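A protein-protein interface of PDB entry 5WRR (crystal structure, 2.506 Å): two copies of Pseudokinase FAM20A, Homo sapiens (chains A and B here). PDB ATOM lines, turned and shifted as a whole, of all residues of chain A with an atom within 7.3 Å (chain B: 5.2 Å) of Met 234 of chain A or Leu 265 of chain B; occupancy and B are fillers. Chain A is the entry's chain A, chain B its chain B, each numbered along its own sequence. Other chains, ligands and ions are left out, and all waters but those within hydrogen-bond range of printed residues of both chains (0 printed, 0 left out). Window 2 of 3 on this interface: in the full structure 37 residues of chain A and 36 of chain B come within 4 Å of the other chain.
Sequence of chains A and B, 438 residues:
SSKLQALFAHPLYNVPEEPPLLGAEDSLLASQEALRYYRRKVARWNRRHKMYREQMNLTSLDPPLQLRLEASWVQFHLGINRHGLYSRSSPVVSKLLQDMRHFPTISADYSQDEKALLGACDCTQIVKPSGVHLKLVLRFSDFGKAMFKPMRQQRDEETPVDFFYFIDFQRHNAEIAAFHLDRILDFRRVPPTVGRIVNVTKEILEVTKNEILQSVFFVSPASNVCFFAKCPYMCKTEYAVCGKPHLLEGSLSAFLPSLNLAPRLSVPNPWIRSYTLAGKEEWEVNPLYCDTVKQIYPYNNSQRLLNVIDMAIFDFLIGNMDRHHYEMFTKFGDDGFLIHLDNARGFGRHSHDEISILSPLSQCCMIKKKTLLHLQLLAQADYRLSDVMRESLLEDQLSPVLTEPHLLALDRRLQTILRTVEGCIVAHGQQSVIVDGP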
ATOM      1  N   GLY A 119     -13.520 -10.965 -14.063  1.00  0.00           N
ATOM      2  CA  GLY A 119     -14.212  -9.739 -13.710  1.00  0.00           C
ATOM      3  C   GLY A 119     -15.593  -9.778 -14.353  1.00  0.00           C
ATOM      4  O   GLY A 119     -15.684  -9.433 -15.531  1.00  0.00           O
ATOM      5  N   ALA A 120     -16.675 -10.164 -13.659  1.00  0.00           N
ATOM      6  CA  ALA A 120     -16.812 -10.379 -12.206  1.00  0.00           C
ATOM      7  C   ALA A 120     -16.382  -9.133 -11.444  1.00  0.00           C
ATOM      8  O   ALA A 120     -15.363  -9.130 -10.756  1.00  0.00           O
ATOM      9  CB  ALA A 120     -16.031 -11.617 -11.737  1.00  0.00           C
ATOM     10  N   CYS A 121     -17.187  -8.082 -11.567  1.00  0.00           N
ATOM     11  CA  CYS A 121     -16.855  -6.778 -11.010  1.00  0.00           C
ATOM     12  C   CYS A 121     -17.404  -6.652  -9.595  1.00  0.00           C
ATOM     13  O   CYS A 121     -18.621  -6.712  -9.383  1.00  0.00           O
ATOM     14  CB  CYS A 121     -17.400  -5.667 -11.908  1.00  0.00           C
ATOM     15  SG  CYS A 121     -16.927  -4.002 -11.414  1.00  0.00           S
ATOM     16  N   ASP A 122     -16.503  -6.472  -8.632  1.00  0.00           N
ATOM     17  CA  ASP A 122     -16.850  -6.219  -7.239  1.00  0.00           C
ATOM     18  C   ASP A 122     -16.046  -5.013  -6.781  1.00  0.00           C
ATOM     19  O   ASP A 122     -14.811  -5.039  -6.823  1.00  0.00           O
ATOM     20  CB  ASP A 122     -16.556  -7.437  -6.358  1.00  0.00           C
ATOM     21  CG  ASP A 122     -16.749  -7.149  -4.881  1.00  0.00           C
ATOM     22  OD1 ASP A 122     -17.751  -6.494  -4.525  1.00  0.00           O
ATOM     23  OD2 ASP A 122     -15.896  -7.577  -4.075  1.00  0.00           O
ATOM     24  N   CYS A 123     -16.740  -3.960  -6.348  1.00  0.00           N
ATOM     25  CA  CYS A 123     -16.053  -2.721  -6.000  1.00  0.00           C
ATOM     26  C   CYS A 123     -15.259  -2.832  -4.705  1.00  0.00           C
ATOM     27  O   CYS A 123     -14.415  -1.972  -4.438  1.00  0.00           O
ATOM     28  CB  CYS A 123     -17.058  -1.571  -5.910  1.00  0.00           C
ATOM     29  SG  CYS A 123     -17.948  -1.261  -7.458  1.00  0.00           S
ATOM     30  N   THR A 124     -15.511  -3.860  -3.893  1.00  0.00           N
ATOM     31  CA  THR A 124     -14.740  -4.034  -2.665  1.00  0.00           C
ATOM     32  C   THR A 124     -13.268  -4.285  -2.972  1.00  0.00           C
ATOM     33  O   THR A 124     -12.381  -3.656  -2.383  1.00  0.00           O
ATOM     34  CB  THR A 124     -15.326  -5.180  -1.839  1.00  0.00           C
ATOM     35  OG1 THR A 124     -16.503  -4.723  -1.161  1.00  0.00           O
ATOM     36  CG2 THR A 124     -14.317  -5.679  -0.814  1.00  0.00           C
ATOM     37  N   VAL A 127     -11.511  -0.786  -4.928  1.00  0.00           N
ATOM     38  CA  VAL A 127     -11.220   0.482  -4.268  1.00  0.00           C
ATOM     39  C   VAL A 127     -10.305   0.216  -3.077  1.00  0.00           C
ATOM     40  O   VAL A 127     -10.226   1.022  -2.142  1.00  0.00           O
ATOM     41  CB  VAL A 127     -12.519   1.200  -3.846  1.00  0.00           C
ATOM     42  CG1 VAL A 127     -12.277   2.690  -3.637  1.00  0.00           C
ATOM     43  CG2 VAL A 127     -13.594   0.999  -4.898  1.00  0.00           C
ATOM     44  N   PRO A 160     -16.209   9.878  -8.962  1.00  0.00           N
ATOM     45  CA  PRO A 160     -17.059  10.337  -7.848  1.00  0.00           C
ATOM     46  C   PRO A 160     -16.815   9.609  -6.540  1.00  0.00           C
ATOM     47  O   PRO A 160     -17.037  10.188  -5.469  1.00  0.00           O
ATOM     48  CB  PRO A 160     -18.482  10.082  -8.370  1.00  0.00           C
ATOM     49  CG  PRO A 160     -18.345  10.025  -9.855  1.00  0.00           C
ATOM     50  CD  PRO A 160     -17.002   9.420 -10.115  1.00  0.00           C
ATOM     51  N   VAL A 161     -16.352   8.359  -6.587  1.00  0.00           N
ATOM     52  CA  VAL A 161     -16.140   7.599  -5.361  1.00  0.00           C
ATOM     53  C   VAL A 161     -14.839   7.983  -4.661  1.00  0.00           C
ATOM     54  O   VAL A 161     -14.745   7.861  -3.432  1.00  0.00           O
ATOM     55  CB  VAL A 161     -16.197   6.094  -5.686  1.00  0.00           C
ATOM     56  CG1 VAL A 161     -15.028   5.332  -5.067  1.00  0.00           C
ATOM     57  CG2 VAL A 161     -17.528   5.504  -5.237  1.00  0.00           C
ATOM     58  N   ALA A 229     -10.246   0.780 -17.824  1.00  0.00           N
ATOM     59  CA  ALA A 229     -10.551  -0.406 -17.035  1.00  0.00           C
ATOM     60  C   ALA A 229     -12.051  -0.427 -16.770  1.00  0.00           C
ATOM     61  O   ALA A 229     -12.601   0.541 -16.232  1.00  0.00           O
ATOM     62  CB  ALA A 229      -9.759  -0.414 -15.727  1.00  0.00           C
ATOM     63  N   LYS A 230     -12.708  -1.524 -17.153  1.00  0.00           N
ATOM     64  CA  LYS A 230     -14.169  -1.559 -17.154  1.00  0.00           C
ATOM     65  C   LYS A 230     -14.737  -1.553 -15.737  1.00  0.00           C
ATOM     66  O   LYS A 230     -15.643  -0.771 -15.426  1.00  0.00           O
ATOM     67  CB  LYS A 230     -14.659  -2.786 -17.922  1.00  0.00           C
ATOM     68  CG  LYS A 230     -16.171  -2.968 -17.901  1.00  0.00           C
ATOM     69  CD  LYS A 230     -16.609  -4.109 -18.808  1.00  0.00           C
ATOM     70  CE  LYS A 230     -18.124  -4.223 -18.851  1.00  0.00           C
ATOM     71  NZ  LYS A 230     -18.578  -5.299 -19.776  1.00  0.00           N
ATOM     72  N   CYS A 231     -14.225  -2.416 -14.865  1.00  0.00           N
ATOM     73  CA  CYS A 231     -14.769  -2.528 -13.516  1.00  0.00           C
ATOM     74  C   CYS A 231     -14.535  -1.257 -12.697  1.00  0.00           C
ATOM     75  O   CYS A 231     -15.457  -0.811 -12.003  1.00  0.00           O
ATOM     76  CB  CYS A 231     -14.199  -3.761 -12.811  1.00  0.00           C
ATOM     77  SG  CYS A 231     -14.908  -4.141 -11.185  1.00  0.00           S
ATOM     78  N   PRO A 232     -13.342  -0.645 -12.724  1.00  0.00           N
ATOM     79  CA  PRO A 232     -13.202   0.661 -12.060  1.00  0.00           C
ATOM     80  C   PRO A 232     -14.156   1.724 -12.584  1.00  0.00           C
ATOM     81  O   PRO A 232     -14.585   2.588 -11.808  1.00  0.00           O
ATOM     82  CB  PRO A 232     -11.736   1.031 -12.330  1.00  0.00           C
ATOM     83  CG  PRO A 232     -11.052  -0.278 -12.400  1.00  0.00           C
ATOM     84  CD  PRO A 232     -12.024  -1.188 -13.110  1.00  0.00           C
ATOM     85  N   TYR A 233     -14.509   1.688 -13.872  1.00  0.00           N
ATOM     86  CA  TYR A 233     -15.441   2.681 -14.402  1.00  0.00           C
ATOM     87  C   TYR A 233     -16.833   2.507 -13.806  1.00  0.00           C
ATOM     88  O   TYR A 233     -17.500   3.495 -13.474  1.00  0.00           O
ATOM     89  CB  TYR A 233     -15.497   2.602 -15.926  1.00  0.00           C
ATOM     90  CG  TYR A 233     -16.661   3.358 -16.524  1.00  0.00           C
ATOM     91  CD1 TYR A 233     -16.625   4.740 -16.643  1.00  0.00           C
ATOM     92  CD2 TYR A 233     -17.793   2.690 -16.974  1.00  0.00           C
ATOM     93  CE1 TYR A 233     -17.686   5.440 -17.189  1.00  0.00           C
ATOM     94  CE2 TYR A 233     -18.860   3.379 -17.523  1.00  0.00           C
ATOM     95  CZ  TYR A 233     -18.801   4.754 -17.629  1.00  0.00           C
ATOM     96  OH  TYR A 233     -19.861   5.442 -18.175  1.00  0.00           O
ATOM     97  N   MET A 234     -17.297   1.261 -13.683  1.00  0.00           N
ATOM     98  CA  MET A 234     -18.591   1.018 -13.055  1.00  0.00           C
ATOM     99  C   MET A 234     -18.571   1.370 -11.573  1.00  0.00           C
ATOM    100  O   MET A 234     -19.596   1.792 -11.025  1.00  0.00           O
ATOM    101  CB  MET A 234     -19.010  -0.438 -13.260  1.00  0.00           C
ATOM    102  CG  MET A 234     -19.342  -0.777 -14.706  1.00  0.00           C
ATOM    103  SD  MET A 234     -19.730  -2.519 -14.969  1.00  0.00           S
ATOM    104  CE  MET A 234     -18.128  -3.274 -14.712  1.00  0.00           C
ATOM    105  N   CYS A 235     -17.426   1.211 -10.912  1.00  0.00           N
ATOM    106  CA  CYS A 235     -17.293   1.573  -9.507  1.00  0.00           C
ATOM    107  C   CYS A 235     -17.042   3.062  -9.300  1.00  0.00           C
ATOM    108  O   CYS A 235     -16.886   3.491  -8.152  1.00  0.00           O
ATOM    109  CB  CYS A 235     -16.168   0.759  -8.862  1.00  0.00           C
ATOM    110  SG  CYS A 235     -16.482  -1.022  -8.854  1.00  0.00           S
ATOM    111  N   LYS A 236     -16.999   3.848 -10.378  1.00  0.00           N
ATOM    112  CA  LYS A 236     -16.893   5.307 -10.307  1.00  0.00           C
ATOM    113  C   LYS A 236     -15.592   5.754  -9.641  1.00  0.00           C
ATOM    114  O   LYS A 236     -15.553   6.753  -8.919  1.00  0.00           O
ATOM    115  CB  LYS A 236     -18.109   5.916  -9.605  1.00  0.00           C
ATOM    116  CG  LYS A 236     -19.430   5.497 -10.230  1.00  0.00           C
ATOM    117  CD  LYS A 236     -20.604   6.281  -9.670  1.00  0.00           C
ATOM    118  CE  LYS A 236     -21.891   5.896 -10.381  1.00  0.00           C
ATOM    119  NZ  LYS A 236     -21.751   5.990 -11.863  1.00  0.00           N
ATOM    120  N   THR A 237     -14.516   5.017  -9.896  1.00  0.00           N
ATOM    121  CA  THR A 237     -13.175   5.395  -9.481  1.00  0.00           C
ATOM    122  C   THR A 237     -12.335   5.658 -10.734  1.00  0.00           C
ATOM    123  O   THR A 237     -12.858   5.709 -11.853  1.00  0.00           O
ATOM    124  CB  THR A 237     -12.565   4.313  -8.580  1.00  0.00           C
ATOM    125  OG1 THR A 237     -11.319   4.774  -8.045  1.00  0.00           O
ATOM    126  CG2 THR A 237     -12.329   3.028  -9.357  1.00  0.00           C
ATOM    127  N   TYR A 239     -10.438   5.293 -13.929  1.00  0.00           N
ATOM    128  CA  TYR A 239     -10.666   4.242 -14.911  1.00  0.00           C
ATOM    129  C   TYR A 239     -10.017   4.465 -16.266  1.00  0.00           C
ATOM    130  O   TYR A 239     -10.085   3.553 -17.093  1.00  0.00           O
ATOM    131  CB  TYR A 239     -12.176   4.038 -15.129  1.00  0.00           C
ATOM    132  CG  TYR A 239     -12.873   5.197 -15.814  1.00  0.00           C
ATOM    133  CD1 TYR A 239     -13.005   5.235 -17.198  1.00  0.00           C
ATOM    134  CD2 TYR A 239     -13.401   6.250 -15.078  1.00  0.00           C
ATOM    135  CE1 TYR A 239     -13.636   6.290 -17.828  1.00  0.00           C
ATOM    136  CE2 TYR A 239     -14.040   7.308 -15.700  1.00  0.00           C
ATOM    137  CZ  TYR A 239     -14.153   7.322 -17.075  1.00  0.00           C
ATOM    138  OH  TYR A 239     -14.784   8.371 -17.699  1.00  0.00           O
ATOM    139  N   PRO B 263     -26.631  -3.452  -7.294  1.00  0.00           N
ATOM    140  CA  PRO B 263     -25.201  -3.130  -7.291  1.00  0.00           C
ATOM    141  C   PRO B 263     -24.835  -2.262  -6.099  1.00  0.00           C
ATOM    142  O   PRO B 263     -25.653  -1.496  -5.581  1.00  0.00           O
ATOM    143  CB  PRO B 263     -24.996  -2.371  -8.611  1.00  0.00           C
ATOM    144  CG  PRO B 263     -26.248  -2.583  -9.404  1.00  0.00           C
ATOM    145  CD  PRO B 263     -27.341  -2.817  -8.414  1.00  0.00           C
ATOM    146  N   ARG B 264     -23.584  -2.384  -5.665  1.00  0.00           N
ATOM    147  CA  ARG B 264     -23.096  -1.630  -4.522  1.00  0.00           C
ATOM    148  C   ARG B 264     -21.839  -0.867  -4.910  1.00  0.00           C
ATOM    149  O   ARG B 264     -21.070  -1.300  -5.772  1.00  0.00           O
ATOM    150  CB  ARG B 264     -22.777  -2.531  -3.313  1.00  0.00           C
ATOM    151  CG  ARG B 264     -23.973  -3.208  -2.669  1.00  0.00           C
ATOM    152  CD  ARG B 264     -23.568  -3.887  -1.361  1.00  0.00           C
ATOM    153  NE  ARG B 264     -22.780  -5.105  -1.544  1.00  0.00           N
ATOM    154  CZ  ARG B 264     -23.293  -6.306  -1.791  1.00  0.00           C
ATOM    155  NH1 ARG B 264     -24.605  -6.465  -1.897  1.00  0.00           N
ATOM    156  NH2 ARG B 264     -22.490  -7.352  -1.935  1.00  0.00           N
ATOM    157  N   LEU B 265     -21.646   0.282  -4.267  1.00  0.00           N
ATOM    158  CA  LEU B 265     -20.425   1.059  -4.381  1.00  0.00           C
ATOM    159  C   LEU B 265     -19.656   0.998  -3.068  1.00  0.00           C
ATOM    160  O   LEU B 265     -20.246   0.935  -1.984  1.00  0.00           O
ATOM    161  CB  LEU B 265     -20.720   2.521  -4.735  1.00  0.00           C
ATOM    162  CG  LEU B 265     -21.353   2.844  -6.090  1.00  0.00           C
ATOM    163  CD1 LEU B 265     -21.645   4.334  -6.187  1.00  0.00           C
ATOM    164  CD2 LEU B 265     -20.453   2.399  -7.232  1.00  0.00           C
ATOM    165  N   SER B 266     -18.333   1.011  -3.180  1.00  0.00           N
ATOM    166  CA  SER B 266     -17.440   1.122  -2.036  1.00  0.00           C
ATOM    167  C   SER B 266     -16.851   2.524  -2.020  1.00  0.00           C
ATOM    168  O   SER B 266     -16.340   2.999  -3.039  1.00  0.00           O
ATOM    169  CB  SER B 266     -16.329   0.065  -2.095  1.00  0.00           C
ATOM    170  OG  SER B 266     -16.852  -1.234  -1.870  1.00  0.00           O
ATOM    171  N   VAL B 267     -16.924   3.182  -0.868  1.00  0.00           N
ATOM    172  CA  VAL B 267     -16.519   4.572  -0.710  1.00  0.00           C
ATOM    173  C   VAL B 267     -15.483   4.643   0.405  1.00  0.00           C
ATOM    174  O   VAL B 267     -15.713   4.095   1.484  1.00  0.00           O
ATOM    175  CB  VAL B 267     -17.708   5.496  -0.384  1.00  0.00           C
ATOM    176  CG1 VAL B 267     -17.275   6.951  -0.367  1.00  0.00           C
ATOM    177  CG2 VAL B 267     -18.840   5.279  -1.373  1.00  0.00           C
ATOM    178  N   TYR B 326     -16.808   2.041   3.330  1.00  0.00           N
ATOM    179  CA  TYR B 326     -18.191   1.677   3.582  1.00  0.00           C
ATOM    180  C   TYR B 326     -18.906   1.484   2.253  1.00  0.00           C
ATOM    181  O   TYR B 326     -18.470   1.983   1.212  1.00  0.00           O
ATOM    182  CB  TYR B 326     -18.908   2.730   4.436  1.00  0.00           C
ATOM    183  CG  TYR B 326     -18.949   4.125   3.849  1.00  0.00           C
ATOM    184  CD1 TYR B 326     -19.950   4.499   2.963  1.00  0.00           C
ATOM    185  CD2 TYR B 326     -18.004   5.077   4.208  1.00  0.00           C
ATOM    186  CE1 TYR B 326     -19.998   5.776   2.434  1.00  0.00           C
ATOM    187  CE2 TYR B 326     -18.047   6.360   3.686  1.00  0.00           C
ATOM    188  CZ  TYR B 326     -19.047   6.702   2.801  1.00  0.00           C
ATOM    189  OH  TYR B 326     -19.095   7.976   2.279  1.00  0.00           O
ATOM    190  N   GLU B 327     -20.011   0.747   2.293  1.00  0.00           N
ATOM    191  CA  GLU B 327     -20.732   0.382   1.086  1.00  0.00           C
ATOM    192  C   GLU B 327     -22.137   0.965   1.101  1.00  0.00           C
ATOM    193  O   GLU B 327     -22.715   1.219   2.161  1.00  0.00           O
ATOM    194  CB  GLU B 327     -20.796  -1.140   0.912  1.00  0.00           C
ATOM    195  CG  GLU B 327     -19.434  -1.777   0.681  1.00  0.00           C
ATOM    196  CD  GLU B 327     -19.523  -3.233   0.273  1.00  0.00           C
ATOM    197  OE1 GLU B 327     -20.419  -3.574  -0.527  1.00  0.00           O
ATOM    198  OE2 GLU B 327     -18.695  -4.035   0.752  1.00  0.00           O
ATOM    199  N   MET B 328     -22.672   1.183  -0.098  1.00  0.00           N
ATOM    200  CA  MET B 328     -24.003   1.737  -0.287  1.00  0.00           C
ATOM    201  C   MET B 328     -24.674   1.019  -1.445  1.00  0.00           C
ATOM    202  O   MET B 328     -24.004   0.489  -2.334  1.00  0.00           O
ATOM    203  CB  MET B 328     -23.968   3.239  -0.597  1.00  0.00           C
ATOM    204  CG  MET B 328     -23.110   4.073   0.329  1.00  0.00           C
ATOM    205  SD  MET B 328     -23.182   5.810  -0.139  1.00  0.00           S
ATOM    206  CE  MET B 328     -24.907   6.172   0.169  1.00  0.00           C
ATOM    207  N   THR B 330     -26.687   1.272  -4.876  1.00  0.00           N
ATOM    208  CA  THR B 330     -26.786   2.246  -5.960  1.00  0.00           C
ATOM    209  C   THR B 330     -28.175   2.873  -6.030  1.00  0.00           C
ATOM    210  O   THR B 330     -28.308   4.083  -6.253  1.00  0.00           O
ATOM    211  CB  THR B 330     -26.436   1.572  -7.289  1.00  0.00           C
ATOM    212  OG1 THR B 330     -25.026   1.326  -7.342  1.00  0.00           O
ATOM    213  CG2 THR B 330     -26.838   2.445  -8.469  1.00  0.00           C
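OE2 of Glu 327 of chain B lies within hydrogen-bond range of OG1 of Thr 124 of chain A, 3.0 Å away.
SG of Cys 123 of chain A lies close to O of Arg 264 of chain B (3.5 Å).
No position is printed for both chains.
Of the 8 pairs that touch across the chains among the printed residues, none has its exchanged pair printed and touching as well.
Among the printed residues, merely in contact across the chains: Cys 123 of chain A with Ser 266 of chain B, Thr 124 of chain A with Ser 266 of chain B, Val 127 of chain A with Ser 266 of chain B, Val 161 of chain A with Ser 266 of chain B, Met 234 of chain A with Leu 265 of chain B and Cys 235 of chain A with Leu 265 of chain B.
Met 234 of chain A touches one residue of chain B.
Of chain A, only Met 234 (3.9 Å) and Cys 235 (3.8 Å) come within 4 Å of Leu 265 of chain B.
Printed residues of chain A within 4 Å of Glu 327 of chain B: Thr 124.
Printed residues of chain B within 4 Å of Thr 124 of chain A: Ser 266 and Glu 327.
Of the printed residues of chain B, Val 161 of chain A touches Ser 266 (3.4 Å).
Gly 119 of chain A touches none of the printed residues of chain B.
The nearest printed residue of chain B that does not touch Met 234 of chain A is Arg 264 of chain B (6.3 Å).
Hydrophobic or aromatic side chains of chain B that line the printed part of chain A: Leu 265.
Hydrophobic or aromatic side chains of chain A within 4 Å of the printed part of chain B: Val 127 and Val 161.
Among the printed residues, no Asp or Glu carboxylate lies within 4 Å of a Lys or Arg side-chain nitrogen of the other chain.
The side-chain sulfur (SG) of Cys 235 of chain A forms a disulfide with the side-chain sulfur (SG) of Cys 123 of chain A, at 2.0 Å.
O of Lys 236 of chain A sits at hydrogen-bond distance from N of Val 161 of chain A (2.9 Å).
NE of Arg 264 of chain B is in salt-bridge range of OE1 of Glu 327 of chain B (3.0 Å).
N of Leu 265 of chain B is in hydrogen-bond range of O of Met 328 of chain B, at 3.1 Å.
The side-chain sulfur (SG) of Cys 121 of chain A is disulfide-bonded to the side-chain sulfur (SG) of Cys 231 of chain A.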
